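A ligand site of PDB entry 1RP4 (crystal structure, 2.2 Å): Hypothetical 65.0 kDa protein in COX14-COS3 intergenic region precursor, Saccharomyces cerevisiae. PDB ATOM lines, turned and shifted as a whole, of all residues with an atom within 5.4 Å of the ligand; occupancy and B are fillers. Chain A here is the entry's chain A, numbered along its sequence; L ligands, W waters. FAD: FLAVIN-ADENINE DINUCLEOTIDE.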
ATOM      1  N   VAL A  69      24.442 -15.679  -2.071  1.00  0.00           N
ATOM      2  CA  VAL A  69      25.353 -16.609  -2.727  1.00  0.00           C
ATOM      3  C   VAL A  69      26.809 -16.213  -2.563  1.00  0.00           C
ATOM      4  O   VAL A  69      27.165 -15.045  -2.664  1.00  0.00           O
ATOM      5  CB  VAL A  69      25.061 -16.689  -4.242  1.00  0.00           C
ATOM      6  CG1 VAL A  69      23.631 -17.127  -4.483  1.00  0.00           C
ATOM      7  CG2 VAL A  69      25.305 -15.343  -4.898  1.00  0.00           C
ATOM      8  N   GLU A 148      14.016  -9.715 -14.684  1.00  0.00           N
ATOM      9  CA  GLU A 148      14.610 -10.802 -13.919  1.00  0.00           C
ATOM     10  C   GLU A 148      16.101 -10.713 -14.239  1.00  0.00           C
ATOM     11  O   GLU A 148      16.464 -10.496 -15.392  1.00  0.00           O
ATOM     12  CB  GLU A 148      14.030 -12.136 -14.386  1.00  0.00           C
ATOM     13  CG  GLU A 148      14.451 -13.349 -13.570  1.00  0.00           C
ATOM     14  CD  GLU A 148      13.758 -14.624 -14.024  1.00  0.00           C
ATOM     15  OE1 GLU A 148      13.969 -15.050 -15.184  1.00  0.00           O
ATOM     16  OE2 GLU A 148      12.994 -15.211 -13.231  1.00  0.00           O
ATOM     17  N   ARG A 149      16.943 -10.866 -13.226  1.00  0.00           N
ATOM     18  CA  ARG A 149      18.390 -10.767 -13.419  1.00  0.00           C
ATOM     19  C   ARG A 149      19.125 -11.348 -12.215  1.00  0.00           C
ATOM     20  O   ARG A 149      18.499 -11.806 -11.261  1.00  0.00           O
ATOM     21  CB  ARG A 149      18.798  -9.296 -13.581  1.00  0.00           C
ATOM     22  CG  ARG A 149      18.561  -8.480 -12.307  1.00  0.00           C
ATOM     23  CD  ARG A 149      18.903  -6.999 -12.430  1.00  0.00           C
ATOM     24  NE  ARG A 149      18.665  -6.303 -11.166  1.00  0.00           N
ATOM     25  CZ  ARG A 149      18.746  -4.978 -10.994  1.00  0.00           C
ATOM     26  NH1 ARG A 149      19.049  -4.189 -12.025  1.00  0.00           N
ATOM     27  NH2 ARG A 149      18.532  -4.438  -9.795  1.00  0.00           N
ATOM     28  N   PHE A 150      20.448 -11.336 -12.264  1.00  0.00           N
ATOM     29  CA  PHE A 150      21.250 -11.824 -11.154  1.00  0.00           C
ATOM     30  C   PHE A 150      21.036 -10.862  -9.993  1.00  0.00           C
ATOM     31  O   PHE A 150      21.238  -9.659 -10.135  1.00  0.00           O
ATOM     32  CB  PHE A 150      22.735 -11.857 -11.528  1.00  0.00           C
ATOM     33  CG  PHE A 150      23.639 -12.209 -10.380  1.00  0.00           C
ATOM     34  CD1 PHE A 150      23.573 -13.464  -9.785  1.00  0.00           C
ATOM     35  CD2 PHE A 150      24.546 -11.283  -9.871  1.00  0.00           C
ATOM     36  CE1 PHE A 150      24.377 -13.793  -8.699  1.00  0.00           C
ATOM     37  CE2 PHE A 150      25.358 -11.596  -8.784  1.00  0.00           C
ATOM     38  CZ  PHE A 150      25.276 -12.862  -8.200  1.00  0.00           C
ATOM     39  N   THR A 151      20.621 -11.386  -8.837  1.00  0.00           N
ATOM     40  CA  THR A 151      20.369 -10.547  -7.666  1.00  0.00           C
ATOM     41  C   THR A 151      21.264 -10.934  -6.495  1.00  0.00           C
ATOM     42  O   THR A 151      21.264 -10.252  -5.463  1.00  0.00           O
ATOM     43  CB  THR A 151      18.903 -10.678  -7.202  1.00  0.00           C
ATOM     44  OG1 THR A 151      18.695 -11.938  -6.559  1.00  0.00           O
ATOM     45  CG2 THR A 151      17.963 -10.569  -8.401  1.00  0.00           C
ATOM     46  N   GLY A 152      22.019 -12.011  -6.640  1.00  0.00           N
ATOM     47  CA  GLY A 152      22.894 -12.443  -5.559  1.00  0.00           C
ATOM     48  C   GLY A 152      22.193 -13.352  -4.565  1.00  0.00           C
ATOM     49  O   GLY A 152      22.817 -13.941  -3.697  1.00  0.00           O
ATOM     50  N   TYR A 153      20.873 -13.468  -4.697  1.00  0.00           N
ATOM     51  CA  TYR A 153      20.077 -14.329  -3.817  1.00  0.00           C
ATOM     52  C   TYR A 153      20.507 -15.796  -3.980  1.00  0.00           C
ATOM     53  O   TYR A 153      20.823 -16.246  -5.091  1.00  0.00           O
ATOM     54  CB  TYR A 153      18.603 -14.182  -4.185  1.00  0.00           C
ATOM     55  CG  TYR A 153      17.672 -15.086  -3.415  1.00  0.00           C
ATOM     56  CD1 TYR A 153      17.453 -14.891  -2.055  1.00  0.00           C
ATOM     57  CD2 TYR A 153      16.969 -16.103  -4.062  1.00  0.00           C
ATOM     58  CE1 TYR A 153      16.552 -15.692  -1.354  1.00  0.00           C
ATOM     59  CE2 TYR A 153      16.068 -16.896  -3.376  1.00  0.00           C
ATOM     60  CZ  TYR A 153      15.863 -16.683  -2.022  1.00  0.00           C
ATOM     61  OH  TYR A 153      14.970 -17.474  -1.341  1.00  0.00           O
ATOM     62  N   GLY A 154      20.516 -16.522  -2.863  1.00  0.00           N
ATOM     63  CA  GLY A 154      20.911 -17.914  -2.888  1.00  0.00           C
ATOM     64  C   GLY A 154      21.030 -18.469  -1.483  1.00  0.00           C
ATOM     65  O   GLY A 154      20.154 -18.255  -0.652  1.00  0.00           O
ATOM     66  N   GLY A 155      22.103 -19.210  -1.222  1.00  0.00           N
ATOM     67  CA  GLY A 155      22.319 -19.783   0.095  1.00  0.00           C
ATOM     68  C   GLY A 155      21.328 -20.828   0.588  1.00  0.00           C
ATOM     69  O   GLY A 155      20.619 -21.444  -0.207  1.00  0.00           O
ATOM     70  N   ALA A 158      17.413 -20.296  -0.405  1.00  0.00           N
ATOM     71  CA  ALA A 158      17.192 -20.590  -1.817  1.00  0.00           C
ATOM     72  C   ALA A 158      17.192 -22.111  -2.011  1.00  0.00           C
ATOM     73  O   ALA A 158      16.297 -22.658  -2.654  1.00  0.00           O
ATOM     74  CB  ALA A 158      18.271 -19.938  -2.650  1.00  0.00           C
ATOM     75  N   GLY A 159      18.195 -22.772  -1.439  1.00  0.00           N
ATOM     76  CA  GLY A 159      18.305 -24.213  -1.557  1.00  0.00           C
ATOM     77  C   GLY A 159      17.161 -24.970  -0.895  1.00  0.00           C
ATOM     78  O   GLY A 159      16.713 -25.988  -1.408  1.00  0.00           O
ATOM     79  N   ILE A 161      14.120 -23.828  -0.481  1.00  0.00           N
ATOM     80  CA  ILE A 161      12.933 -23.604  -1.276  1.00  0.00           C
ATOM     81  C   ILE A 161      12.937 -24.550  -2.479  1.00  0.00           C
ATOM     82  O   ILE A 161      11.961 -25.262  -2.698  1.00  0.00           O
ATOM     83  CB  ILE A 161      12.854 -22.134  -1.729  1.00  0.00           C
ATOM     84  CG1 ILE A 161      12.702 -21.236  -0.491  1.00  0.00           C
ATOM     85  CG2 ILE A 161      11.667 -21.938  -2.670  1.00  0.00           C
ATOM     86  CD1 ILE A 161      12.530 -19.766  -0.801  1.00  0.00           C
ATOM     87  N   TRP A 162      14.033 -24.589  -3.226  1.00  0.00           N
ATOM     88  CA  TRP A 162      14.133 -25.492  -4.375  1.00  0.00           C
ATOM     89  C   TRP A 162      13.938 -26.955  -3.952  1.00  0.00           C
ATOM     90  O   TRP A 162      13.230 -27.702  -4.629  1.00  0.00           O
ATOM     91  CB  TRP A 162      15.488 -25.334  -5.083  1.00  0.00           C
ATOM     92  CG  TRP A 162      15.572 -24.119  -5.950  1.00  0.00           C
ATOM     93  CD1 TRP A 162      16.539 -23.148  -5.924  1.00  0.00           C
ATOM     94  CD2 TRP A 162      14.655 -23.732  -6.987  1.00  0.00           C
ATOM     95  NE1 TRP A 162      16.273 -22.188  -6.867  1.00  0.00           N
ATOM     96  CE2 TRP A 162      15.121 -22.518  -7.534  1.00  0.00           C
ATOM     97  CE3 TRP A 162      13.469 -24.294  -7.491  1.00  0.00           C
ATOM     98  CZ2 TRP A 162      14.445 -21.849  -8.567  1.00  0.00           C
ATOM     99  CZ3 TRP A 162      12.789 -23.617  -8.526  1.00  0.00           C
ATOM    100  CH2 TRP A 162      13.288 -22.413  -9.047  1.00  0.00           C
ATOM    101  N   TYR A 166      11.026 -29.616  -5.216  1.00  0.00           N
ATOM    102  CA  TYR A 166      11.337 -30.919  -5.838  1.00  0.00           C
ATOM    103  C   TYR A 166      10.882 -32.090  -4.973  1.00  0.00           C
ATOM    104  O   TYR A 166      10.410 -33.110  -5.486  1.00  0.00           O
ATOM    105  CB  TYR A 166      12.842 -31.048  -6.085  1.00  0.00           C
ATOM    106  CG  TYR A 166      13.380 -30.250  -7.249  1.00  0.00           C
ATOM    107  CD1 TYR A 166      14.262 -29.195  -7.042  1.00  0.00           C
ATOM    108  CD2 TYR A 166      13.030 -30.564  -8.563  1.00  0.00           C
ATOM    109  CE1 TYR A 166      14.793 -28.467  -8.104  1.00  0.00           C
ATOM    110  CE2 TYR A 166      13.557 -29.833  -9.649  1.00  0.00           C
ATOM    111  CZ  TYR A 166      14.428 -28.786  -9.407  1.00  0.00           C
ATOM    112  OH  TYR A 166      14.939 -28.050 -10.439  1.00  0.00           O
ATOM    113  N   TYR A 186       8.439 -32.771 -12.362  1.00  0.00           N
ATOM    114  CA  TYR A 186       9.877 -32.563 -12.213  1.00  0.00           C
ATOM    115  C   TYR A 186      10.488 -31.761 -13.378  1.00  0.00           C
ATOM    116  O   TYR A 186      11.256 -30.850 -13.174  1.00  0.00           O
ATOM    117  CB  TYR A 186      10.590 -33.910 -12.097  1.00  0.00           C
ATOM    118  CG  TYR A 186      12.089 -33.772 -12.249  1.00  0.00           C
ATOM    119  CD1 TYR A 186      12.872 -33.307 -11.201  1.00  0.00           C
ATOM    120  CD2 TYR A 186      12.702 -34.012 -13.480  1.00  0.00           C
ATOM    121  CE1 TYR A 186      14.234 -33.086 -11.379  1.00  0.00           C
ATOM    122  CE2 TYR A 186      14.065 -33.792 -13.658  1.00  0.00           C
ATOM    123  CZ  TYR A 186      14.815 -33.331 -12.605  1.00  0.00           C
ATOM    124  OH  TYR A 186      16.161 -33.096 -12.782  1.00  0.00           O
ATOM    125  N   VAL A 189       9.463 -28.069 -13.248  1.00  0.00           N
ATOM    126  CA  VAL A 189      10.225 -27.339 -12.219  1.00  0.00           C
ATOM    127  C   VAL A 189      11.683 -27.136 -12.657  1.00  0.00           C
ATOM    128  O   VAL A 189      12.241 -26.056 -12.488  1.00  0.00           O
ATOM    129  CB  VAL A 189      10.199 -28.088 -10.851  1.00  0.00           C
ATOM    130  CG1 VAL A 189      11.084 -27.364  -9.830  1.00  0.00           C
ATOM    131  CG2 VAL A 189       8.755 -28.161 -10.305  1.00  0.00           C
ATOM    132  N   SER A 190      12.279 -28.178 -13.223  1.00  0.00           N
ATOM    133  CA  SER A 190      13.660 -28.123 -13.667  1.00  0.00           C
ATOM    134  C   SER A 190      13.853 -27.077 -14.781  1.00  0.00           C
ATOM    135  O   SER A 190      14.819 -26.316 -14.755  1.00  0.00           O
ATOM    136  CB  SER A 190      14.092 -29.505 -14.171  1.00  0.00           C
ATOM    137  OG  SER A 190      15.431 -29.501 -14.593  1.00  0.00           O
ATOM    138  N   GLY A 191      12.936 -27.031 -15.737  1.00  0.00           N
ATOM    139  CA  GLY A 191      13.047 -26.051 -16.801  1.00  0.00           C
ATOM    140  C   GLY A 191      12.914 -24.651 -16.218  1.00  0.00           C
ATOM    141  O   GLY A 191      13.572 -23.707 -16.680  1.00  0.00           O
ATOM    142  N   PHE A 192      12.054 -24.512 -15.219  1.00  0.00           N
ATOM    143  CA  PHE A 192      11.810 -23.242 -14.551  1.00  0.00           C
ATOM    144  C   PHE A 192      13.081 -22.815 -13.807  1.00  0.00           C
ATOM    145  O   PHE A 192      13.549 -21.679 -13.946  1.00  0.00           O
ATOM    146  CB  PHE A 192      10.602 -23.398 -13.608  1.00  0.00           C
ATOM    147  CG  PHE A 192      10.474 -22.327 -12.559  1.00  0.00           C
ATOM    148  CD1 PHE A 192      10.596 -20.972 -12.889  1.00  0.00           C
ATOM    149  CD2 PHE A 192      10.162 -22.674 -11.251  1.00  0.00           C
ATOM    150  CE1 PHE A 192      10.402 -19.982 -11.925  1.00  0.00           C
ATOM    151  CE2 PHE A 192       9.969 -21.691 -10.271  1.00  0.00           C
ATOM    152  CZ  PHE A 192      10.086 -20.341 -10.609  1.00  0.00           C
ATOM    153  N   HIS A 193      13.654 -23.753 -13.050  1.00  0.00           N
ATOM    154  CA  HIS A 193      14.880 -23.549 -12.267  1.00  0.00           C
ATOM    155  C   HIS A 193      16.034 -23.157 -13.221  1.00  0.00           C
ATOM    156  O   HIS A 193      16.797 -22.221 -12.955  1.00  0.00           O
ATOM    157  CB  HIS A 193      15.209 -24.875 -11.555  1.00  0.00           C
ATOM    158  CG  HIS A 193      16.216 -24.752 -10.450  1.00  0.00           C
ATOM    159  ND1 HIS A 193      16.526 -25.799  -9.618  1.00  0.00           N
ATOM    160  CD2 HIS A 193      16.984 -23.707 -10.046  1.00  0.00           C
ATOM    161  CE1 HIS A 193      17.434 -25.418  -8.747  1.00  0.00           C
ATOM    162  NE2 HIS A 193      17.737 -24.151  -8.984  1.00  0.00           N
ATOM    163  N   ALA A 194      16.129 -23.887 -14.323  1.00  0.00           N
ATOM    164  CA  ALA A 194      17.156 -23.658 -15.327  1.00  0.00           C
ATOM    165  C   ALA A 194      16.944 -22.292 -15.993  1.00  0.00           C
ATOM    166  O   ALA A 194      17.904 -21.546 -16.227  1.00  0.00           O
ATOM    167  CB  ALA A 194      17.111 -24.776 -16.378  1.00  0.00           C
ATOM    168  N   ILE A 196      15.712 -19.620 -14.757  1.00  0.00           N
ATOM    169  CA  ILE A 196      16.214 -18.587 -13.860  1.00  0.00           C
ATOM    170  C   ILE A 196      17.751 -18.580 -13.875  1.00  0.00           C
ATOM    171  O   ILE A 196      18.372 -17.523 -13.923  1.00  0.00           O
ATOM    172  CB  ILE A 196      15.681 -18.836 -12.434  1.00  0.00           C
ATOM    173  CG1 ILE A 196      14.170 -18.582 -12.409  1.00  0.00           C
ATOM    174  CG2 ILE A 196      16.401 -17.939 -11.436  1.00  0.00           C
ATOM    175  CD1 ILE A 196      13.477 -19.082 -11.167  1.00  0.00           C
ATOM    176  N   LEU A 200      20.119 -15.283 -14.787  1.00  0.00           N
ATOM    177  CA  LEU A 200      21.079 -14.673 -13.865  1.00  0.00           C
ATOM    178  C   LEU A 200      22.494 -14.751 -14.441  1.00  0.00           C
ATOM    179  O   LEU A 200      23.368 -13.983 -14.066  1.00  0.00           O
ATOM    180  CB  LEU A 200      20.991 -15.336 -12.488  1.00  0.00           C
ATOM    181  CG  LEU A 200      21.284 -16.826 -12.325  1.00  0.00           C
ATOM    182  CD1 LEU A 200      22.788 -17.050 -12.177  1.00  0.00           C
ATOM    183  CD2 LEU A 200      20.551 -17.339 -11.094  1.00  0.00           C
ATOM    184  N   ARG A 222      25.940 -23.362 -14.241  1.00  0.00           N
ATOM    185  CA  ARG A 222      24.533 -23.561 -13.893  1.00  0.00           C
ATOM    186  C   ARG A 222      23.752 -24.266 -15.011  1.00  0.00           C
ATOM    187  O   ARG A 222      22.711 -24.874 -14.749  1.00  0.00           O
ATOM    188  CB  ARG A 222      23.870 -22.212 -13.616  1.00  0.00           C
ATOM    189  CG  ARG A 222      24.490 -21.394 -12.491  1.00  0.00           C
ATOM    190  CD  ARG A 222      24.446 -22.127 -11.159  1.00  0.00           C
ATOM    191  NE  ARG A 222      24.876 -21.277 -10.056  1.00  0.00           N
ATOM    192  CZ  ARG A 222      24.139 -20.290  -9.540  1.00  0.00           C
ATOM    193  NH1 ARG A 222      22.919 -20.035 -10.015  1.00  0.00           N
ATOM    194  NH2 ARG A 222      24.627 -19.566  -8.547  1.00  0.00           N
ATOM    195  N   ARG A 229      19.248 -29.793 -18.358  1.00  0.00           N
ATOM    196  CA  ARG A 229      18.572 -28.590 -17.899  1.00  0.00           C
ATOM    197  C   ARG A 229      18.161 -27.808 -19.133  1.00  0.00           C
ATOM    198  O   ARG A 229      17.124 -27.136 -19.154  1.00  0.00           O
ATOM    199  CB  ARG A 229      19.503 -27.756 -16.995  1.00  0.00           C
ATOM    200  CG  ARG A 229      19.991 -28.541 -15.798  1.00  0.00           C
ATOM    201  CD  ARG A 229      20.871 -27.749 -14.860  1.00  0.00           C
ATOM    202  NE  ARG A 229      21.243 -28.573 -13.707  1.00  0.00           N
ATOM    203  CZ  ARG A 229      22.040 -28.177 -12.729  1.00  0.00           C
ATOM    204  NH1 ARG A 229      22.567 -26.963 -12.740  1.00  0.00           N
ATOM    205  NH2 ARG A 229      22.312 -29.001 -11.725  1.00  0.00           N
ATOM    206  N   ASN A 232      15.092 -29.476 -20.511  1.00  0.00           N
ATOM    207  CA  ASN A 232      13.891 -29.160 -19.735  1.00  0.00           C
ATOM    208  C   ASN A 232      13.336 -27.785 -20.066  1.00  0.00           C
ATOM    209  O   ASN A 232      12.122 -27.575 -20.016  1.00  0.00           O
ATOM    210  CB  ASN A 232      14.205 -29.319 -18.240  1.00  0.00           C
ATOM    211  CG  ASN A 232      14.515 -30.772 -17.884  1.00  0.00           C
ATOM    212  OD1 ASN A 232      15.156 -31.068 -16.871  1.00  0.00           O
ATOM    213  ND2 ASN A 232      14.043 -31.680 -18.726  1.00  0.00           N
ATOM    214  N   MET A 309       6.315 -19.279  -2.926  1.00  0.00           N
ATOM    215  CA  MET A 309       7.091 -18.195  -3.494  1.00  0.00           C
ATOM    216  C   MET A 309       7.166 -17.038  -2.491  1.00  0.00           C
ATOM    217  O   MET A 309       8.048 -16.184  -2.559  1.00  0.00           O
ATOM    218  CB  MET A 309       6.449 -17.756  -4.804  1.00  0.00           C
ATOM    219  CG  MET A 309       7.463 -17.387  -5.826  1.00  0.00           C
ATOM    220  SD  MET A 309       8.340 -18.900  -6.675  1.00  0.00           S
ATOM    221  CE  MET A 309       8.825 -20.129  -5.254  1.00  0.00           C
ATOM    222  N   VAL A 312      10.387 -16.503  -0.503  1.00  0.00           N
ATOM    223  CA  VAL A 312      11.565 -15.965  -1.177  1.00  0.00           C
ATOM    224  C   VAL A 312      11.764 -14.538  -0.684  1.00  0.00           C
ATOM    225  O   VAL A 312      10.890 -13.695  -0.875  1.00  0.00           O
ATOM    226  CB  VAL A 312      11.365 -15.941  -2.705  1.00  0.00           C
ATOM    227  CG1 VAL A 312      12.607 -15.394  -3.390  1.00  0.00           C
ATOM    228  CG2 VAL A 312      11.062 -17.345  -3.209  1.00  0.00           C
ATOM    229  N   CYS A 314      14.244 -12.341  -1.662  1.00  0.00           N
ATOM    230  CA  CYS A 314      14.536 -11.468  -2.794  1.00  0.00           C
ATOM    231  C   CYS A 314      13.218 -11.129  -3.500  1.00  0.00           C
ATOM    232  O   CYS A 314      12.522 -12.027  -3.980  1.00  0.00           O
ATOM    233  CB  CYS A 314      15.531 -12.162  -3.740  1.00  0.00           C
ATOM    234  SG  CYS A 314      15.521 -11.576  -5.472  1.00  0.00           S
ATOM    235  N   ARG A 316      12.496  -9.235  -6.424  1.00  0.00           N
ATOM    236  CA  ARG A 316      12.406  -9.455  -7.865  1.00  0.00           C
ATOM    237  C   ARG A 316      12.300 -10.957  -8.167  1.00  0.00           C
ATOM    238  O   ARG A 316      11.541 -11.368  -9.058  1.00  0.00           O
ATOM    239  CB  ARG A 316      13.600  -8.790  -8.577  1.00  0.00           C
ATOM    240  CG  ARG A 316      13.372  -7.280  -8.708  1.00  0.00           C
ATOM    241  CD  ARG A 316      14.626  -6.461  -8.915  1.00  0.00           C
ATOM    242  NE  ARG A 316      15.064  -6.405 -10.303  1.00  0.00           N
ATOM    243  CZ  ARG A 316      15.532  -5.306 -10.890  1.00  0.00           C
ATOM    244  NH1 ARG A 316      15.599  -4.167 -10.205  1.00  0.00           N
ATOM    245  NH2 ARG A 316      15.936  -5.340 -12.152  1.00  0.00           N
ATOM    246  N   CYS A 317      13.033 -11.771  -7.405  1.00  0.00           N
ATOM    247  CA  CYS A 317      12.987 -13.208  -7.585  1.00  0.00           C
ATOM    248  C   CYS A 317      11.568 -13.706  -7.283  1.00  0.00           C
ATOM    249  O   CYS A 317      11.048 -14.577  -7.974  1.00  0.00           O
ATOM    250  CB  CYS A 317      13.950 -13.919  -6.634  1.00  0.00           C
ATOM    251  SG  CYS A 317      15.665 -13.302  -6.602  1.00  0.00           S
ATOM    252  N   GLY A 321       9.022 -15.326  -9.853  1.00  0.00           N
ATOM    253  CA  GLY A 321       8.681 -16.681  -9.477  1.00  0.00           C
ATOM    254  C   GLY A 321       7.174 -16.803  -9.514  1.00  0.00           C
ATOM    255  O   GLY A 321       6.630 -17.783 -10.037  1.00  0.00           O
HETATM  256  PA  FAD L   1      21.037 -23.851  -7.601  1.00  0.00           P
HETATM  257  O1A FAD L   1      19.697 -23.291  -7.254  1.00  0.00           O
HETATM  258  O2A FAD L   1      21.846 -23.597  -8.819  1.00  0.00           O
HETATM  259  O5B FAD L   1      21.024 -25.336  -7.106  1.00  0.00           O
HETATM  260  C5B FAD L   1      20.011 -26.116  -6.447  1.00  0.00           C
HETATM  261  C4B FAD L   1      20.510 -27.536  -6.484  1.00  0.00           C
HETATM  262  O4B FAD L   1      19.583 -28.095  -7.460  1.00  0.00           O
HETATM  263  C3B FAD L   1      21.928 -27.983  -6.915  1.00  0.00           C
HETATM  264  O3B FAD L   1      22.074 -29.181  -6.145  1.00  0.00           O
HETATM  265  C2B FAD L   1      21.874 -28.207  -8.360  1.00  0.00           C
HETATM  266  O2B FAD L   1      22.685 -29.293  -8.650  1.00  0.00           O
HETATM  267  C1B FAD L   1      20.372 -28.400  -8.633  1.00  0.00           C
HETATM  268  N9A FAD L   1      19.848 -27.684  -9.752  1.00  0.00           N
HETATM  269  C8A FAD L   1      20.172 -26.447 -10.366  1.00  0.00           C
HETATM  270  N7A FAD L   1      19.519 -26.112 -11.430  1.00  0.00           N
HETATM  271  C5A FAD L   1      18.751 -27.251 -11.699  1.00  0.00           C
HETATM  272  C6A FAD L   1      17.803 -27.590 -12.683  1.00  0.00           C
HETATM  273  N6A FAD L   1      17.409 -26.674 -13.577  1.00  0.00           N
HETATM  274  N1A FAD L   1      17.238 -28.850 -12.678  1.00  0.00           N
HETATM  275  C2A FAD L   1      17.472 -29.833 -11.757  1.00  0.00           C
HETATM  276  N3A FAD L   1      18.310 -29.406 -10.704  1.00  0.00           N
HETATM  277  C4A FAD L   1      18.947 -28.135 -10.725  1.00  0.00           C
HETATM  278  N1  FAD L   1      18.688 -15.711  -8.199  1.00  0.00           N
HETATM  279  C2  FAD L   1      19.102 -14.644  -8.975  1.00  0.00           C
HETATM  280  O2  FAD L   1      20.303 -14.276  -9.017  1.00  0.00           O
HETATM  281  N3  FAD L   1      18.040 -14.167  -9.731  1.00  0.00           N
HETATM  282  C4  FAD L   1      16.716 -14.662  -9.698  1.00  0.00           C
HETATM  283  O4  FAD L   1      15.855 -14.026 -10.389  1.00  0.00           O
HETATM  284  C4X FAD L   1      16.380 -15.722  -8.876  1.00  0.00           C
HETATM  285  N5  FAD L   1      15.060 -16.261  -8.711  1.00  0.00           N
HETATM  286  C5X FAD L   1      14.690 -17.344  -7.861  1.00  0.00           C
HETATM  287  C6  FAD L   1      13.337 -17.776  -7.798  1.00  0.00           C
HETATM  288  C7  FAD L   1      13.044 -18.826  -6.892  1.00  0.00           C
HETATM  289  C7M FAD L   1      11.582 -19.212  -7.095  1.00  0.00           C
HETATM  290  C8  FAD L   1      13.992 -19.438  -6.022  1.00  0.00           C
HETATM  291  C8M FAD L   1      14.001 -20.531  -4.970  1.00  0.00           C
HETATM  292  C9  FAD L   1      15.315 -19.016  -6.151  1.00  0.00           C
HETATM  293  C9A FAD L   1      15.745 -17.973  -7.010  1.00  0.00           C
HETATM  294  N10 FAD L   1      17.046 -17.357  -7.329  1.00  0.00           N
HETATM  295  C10 FAD L   1      17.443 -16.288  -8.111  1.00  0.00           C
HETATM  296  C1' FAD L   1      18.134 -18.190  -6.965  1.00  0.00           C
HETATM  297  C2' FAD L   1      18.869 -19.166  -7.831  1.00  0.00           C
HETATM  298  O2' FAD L   1      17.819 -20.080  -8.265  1.00  0.00           O
HETATM  299  C3' FAD L   1      19.884 -19.979  -7.061  1.00  0.00           C
HETATM  300  O3' FAD L   1      19.242 -20.705  -6.032  1.00  0.00           O
HETATM  301  C4' FAD L   1      21.157 -19.251  -6.638  1.00  0.00           C
HETATM  302  O4' FAD L   1      21.867 -18.585  -7.729  1.00  0.00           O
HETATM  303  C5' FAD L   1      22.134 -20.044  -5.896  1.00  0.00           C
HETATM  304  O5' FAD L   1      22.786 -21.108  -6.614  1.00  0.00           O
HETATM  305  P   FAD L   1      23.114 -22.512  -6.020  1.00  0.00           P
HETATM  306  O1P FAD L   1      24.248 -22.693  -6.897  1.00  0.00           O
HETATM  307  O2P FAD L   1      23.178 -22.466  -4.524  1.00  0.00           O
HETATM  308  O3P FAD L   1      21.821 -23.420  -6.290  1.00  0.00           O
HETATM  309  O   HOH W   1      15.427 -11.378 -10.751  1.00  0.00           O
HETATM  310  O   HOH W   2      18.685 -20.851 -10.781  1.00  0.00           O
HETATM  311  O   HOH W   3      20.870 -22.315 -11.198  1.00  0.00           O
HETATM  312  O   HOH W   4      21.866 -15.647  -7.419  1.00  0.00           O
HETATM  313  O   HOH W   5      12.666 -15.480 -10.491  1.00  0.00           O
HETATM  314  O   HOH W   6      24.012 -20.313  -3.063  1.00  0.00           O
HETATM  315  O   HOH W   7      20.334 -23.913 -13.283  1.00  0.00           O
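O of Ser 190 is in hydrogen-bond range of N6A of the ligand.
The side-chain hydroxyl (OG) of Ser 190 is in hydrogen-bond range of a nitrogen (N1A) of the ligand, at 2.7 Å.
A ring nitrogen (NE2) of His 193 is in hydrogen-bond range of an oxygen (O1A) of the ligand.
O of Arg 149 lies within hydrogen-bond range of N3 of the ligand, at 2.9 Å.
An oxygen (O1P) of the ligand is in salt-bridge range of the guanidinium group (NE) of Arg 222 (3.5 Å).
O2 of the ligand is in hydrogen-bond range of N of Thr 151, at 2.9 Å.
The indole nitrogen (NE1) of Trp 162 lies within hydrogen-bond range of an oxygen (O2') of the ligand (3.0 Å).
NH2 of Arg 229 is in hydrogen-bond range of O2B of the ligand (3.1 Å).
OH of Tyr 166 lies within hydrogen-bond range of N1A of the ligand.
The side-chain amide oxygen of Asn 232 sits at hydrogen-bond distance from the side-chain hydroxyl of Ser 190.
A ring nitrogen (NE2) of His 193 is in hydrogen-bond range of the indole nitrogen (NE1) of Trp 162 (3.2 Å).
The side-chain hydroxyl (OH) of Tyr 166 sits at hydrogen-bond distance from a ring nitrogen (ND1) of His 193, at 2.9 Å.
NH1 of Arg 229 lies within hydrogen-bond range of O of Arg 222 (2.9 Å).
The side-chain sulfur (SG) of Cys 317 is in hydrogen-bond range of the side-chain hydroxyl (OG1) of Thr 151 (3.3 Å).
OG1 of Thr 151 sits at hydrogen-bond distance from SG of Cys 314, at 3.4 Å.
The side-chain sulfur (SG) of Cys 317 forms a disulfide with the side-chain sulfur (SG) of Cys 314.
The backbone NH of Val 69 is in hydrogen-bond range of the backbone carbonyl oxygen of Gly 152 (2.9 Å).
The backbone NH of Ala 194 sits close to a nitrogen (N6A) of the ligand (3.2 Å).
The side-chain sulfur of Cys 317 sits close to a nitrogen (N5) of the ligand (3.7 Å).
Residues that only touch the ligand: Val 69 (3.6 Å), Glu 148 (3.5 Å), Phe 150 (3.4 Å), Gly 152 (3.7 Å), Tyr 153 (3.4 Å), Gly 154 (3.9 Å), Ala 158 (3.6 Å), Ile 161 (3.6 Å), Tyr 186 (3.7 Å), Phe 192 (3.98 Å), Ile 196 (3.4 Å), Leu 200 (3.7 Å) and Met 309 (3.3 Å).
Hydrophobic or aromatic side chains within 4 Å of the ligand: Val 69, Phe 150, Tyr 153, Ala 158, Ile 161, Trp 162, Tyr 166, Phe 192, His 193, Ala 194, Ile 196, Leu 200 and Met 309.
23 residues have an atom within 4 Å of the ligand: Val 69, Glu 148, Arg 149, Phe 150, Thr 151, Gly 152, Tyr 153, Gly 154, Ala 158, Ile 161, Trp 162, Tyr 166, Tyr 186, Ser 190, Phe 192, His 193, Ala 194, Ile 196, Leu 200, Arg 222, Arg 229, Met 309 and Cys 317.
Water W4 bridges O of Tyr 153 and O2 of the ligand.
Water W1 lies within hydrogen-bond range of O4 of the ligand (2.7 Å) and N of Arg 149 (2.9 Å).
Water W6 bridges an oxygen (O2P) of the ligand (2.7 Å) and the backbone NH (N) of Gly 155 (2.9 Å).
Water W2 lies within hydrogen-bond range of an oxygen (O2') of the ligand (2.8 Å) and the backbone carbonyl oxygen (O) of His 193 (3.2 Å).
Water W3 bridges O2A of the ligand and NH1 of Arg 222.
Water W7 lies within hydrogen-bond range of the backbone carbonyl oxygen of Arg 222 (3.0 Å) and a nitrogen (N7A) of the ligand (3.0 Å).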
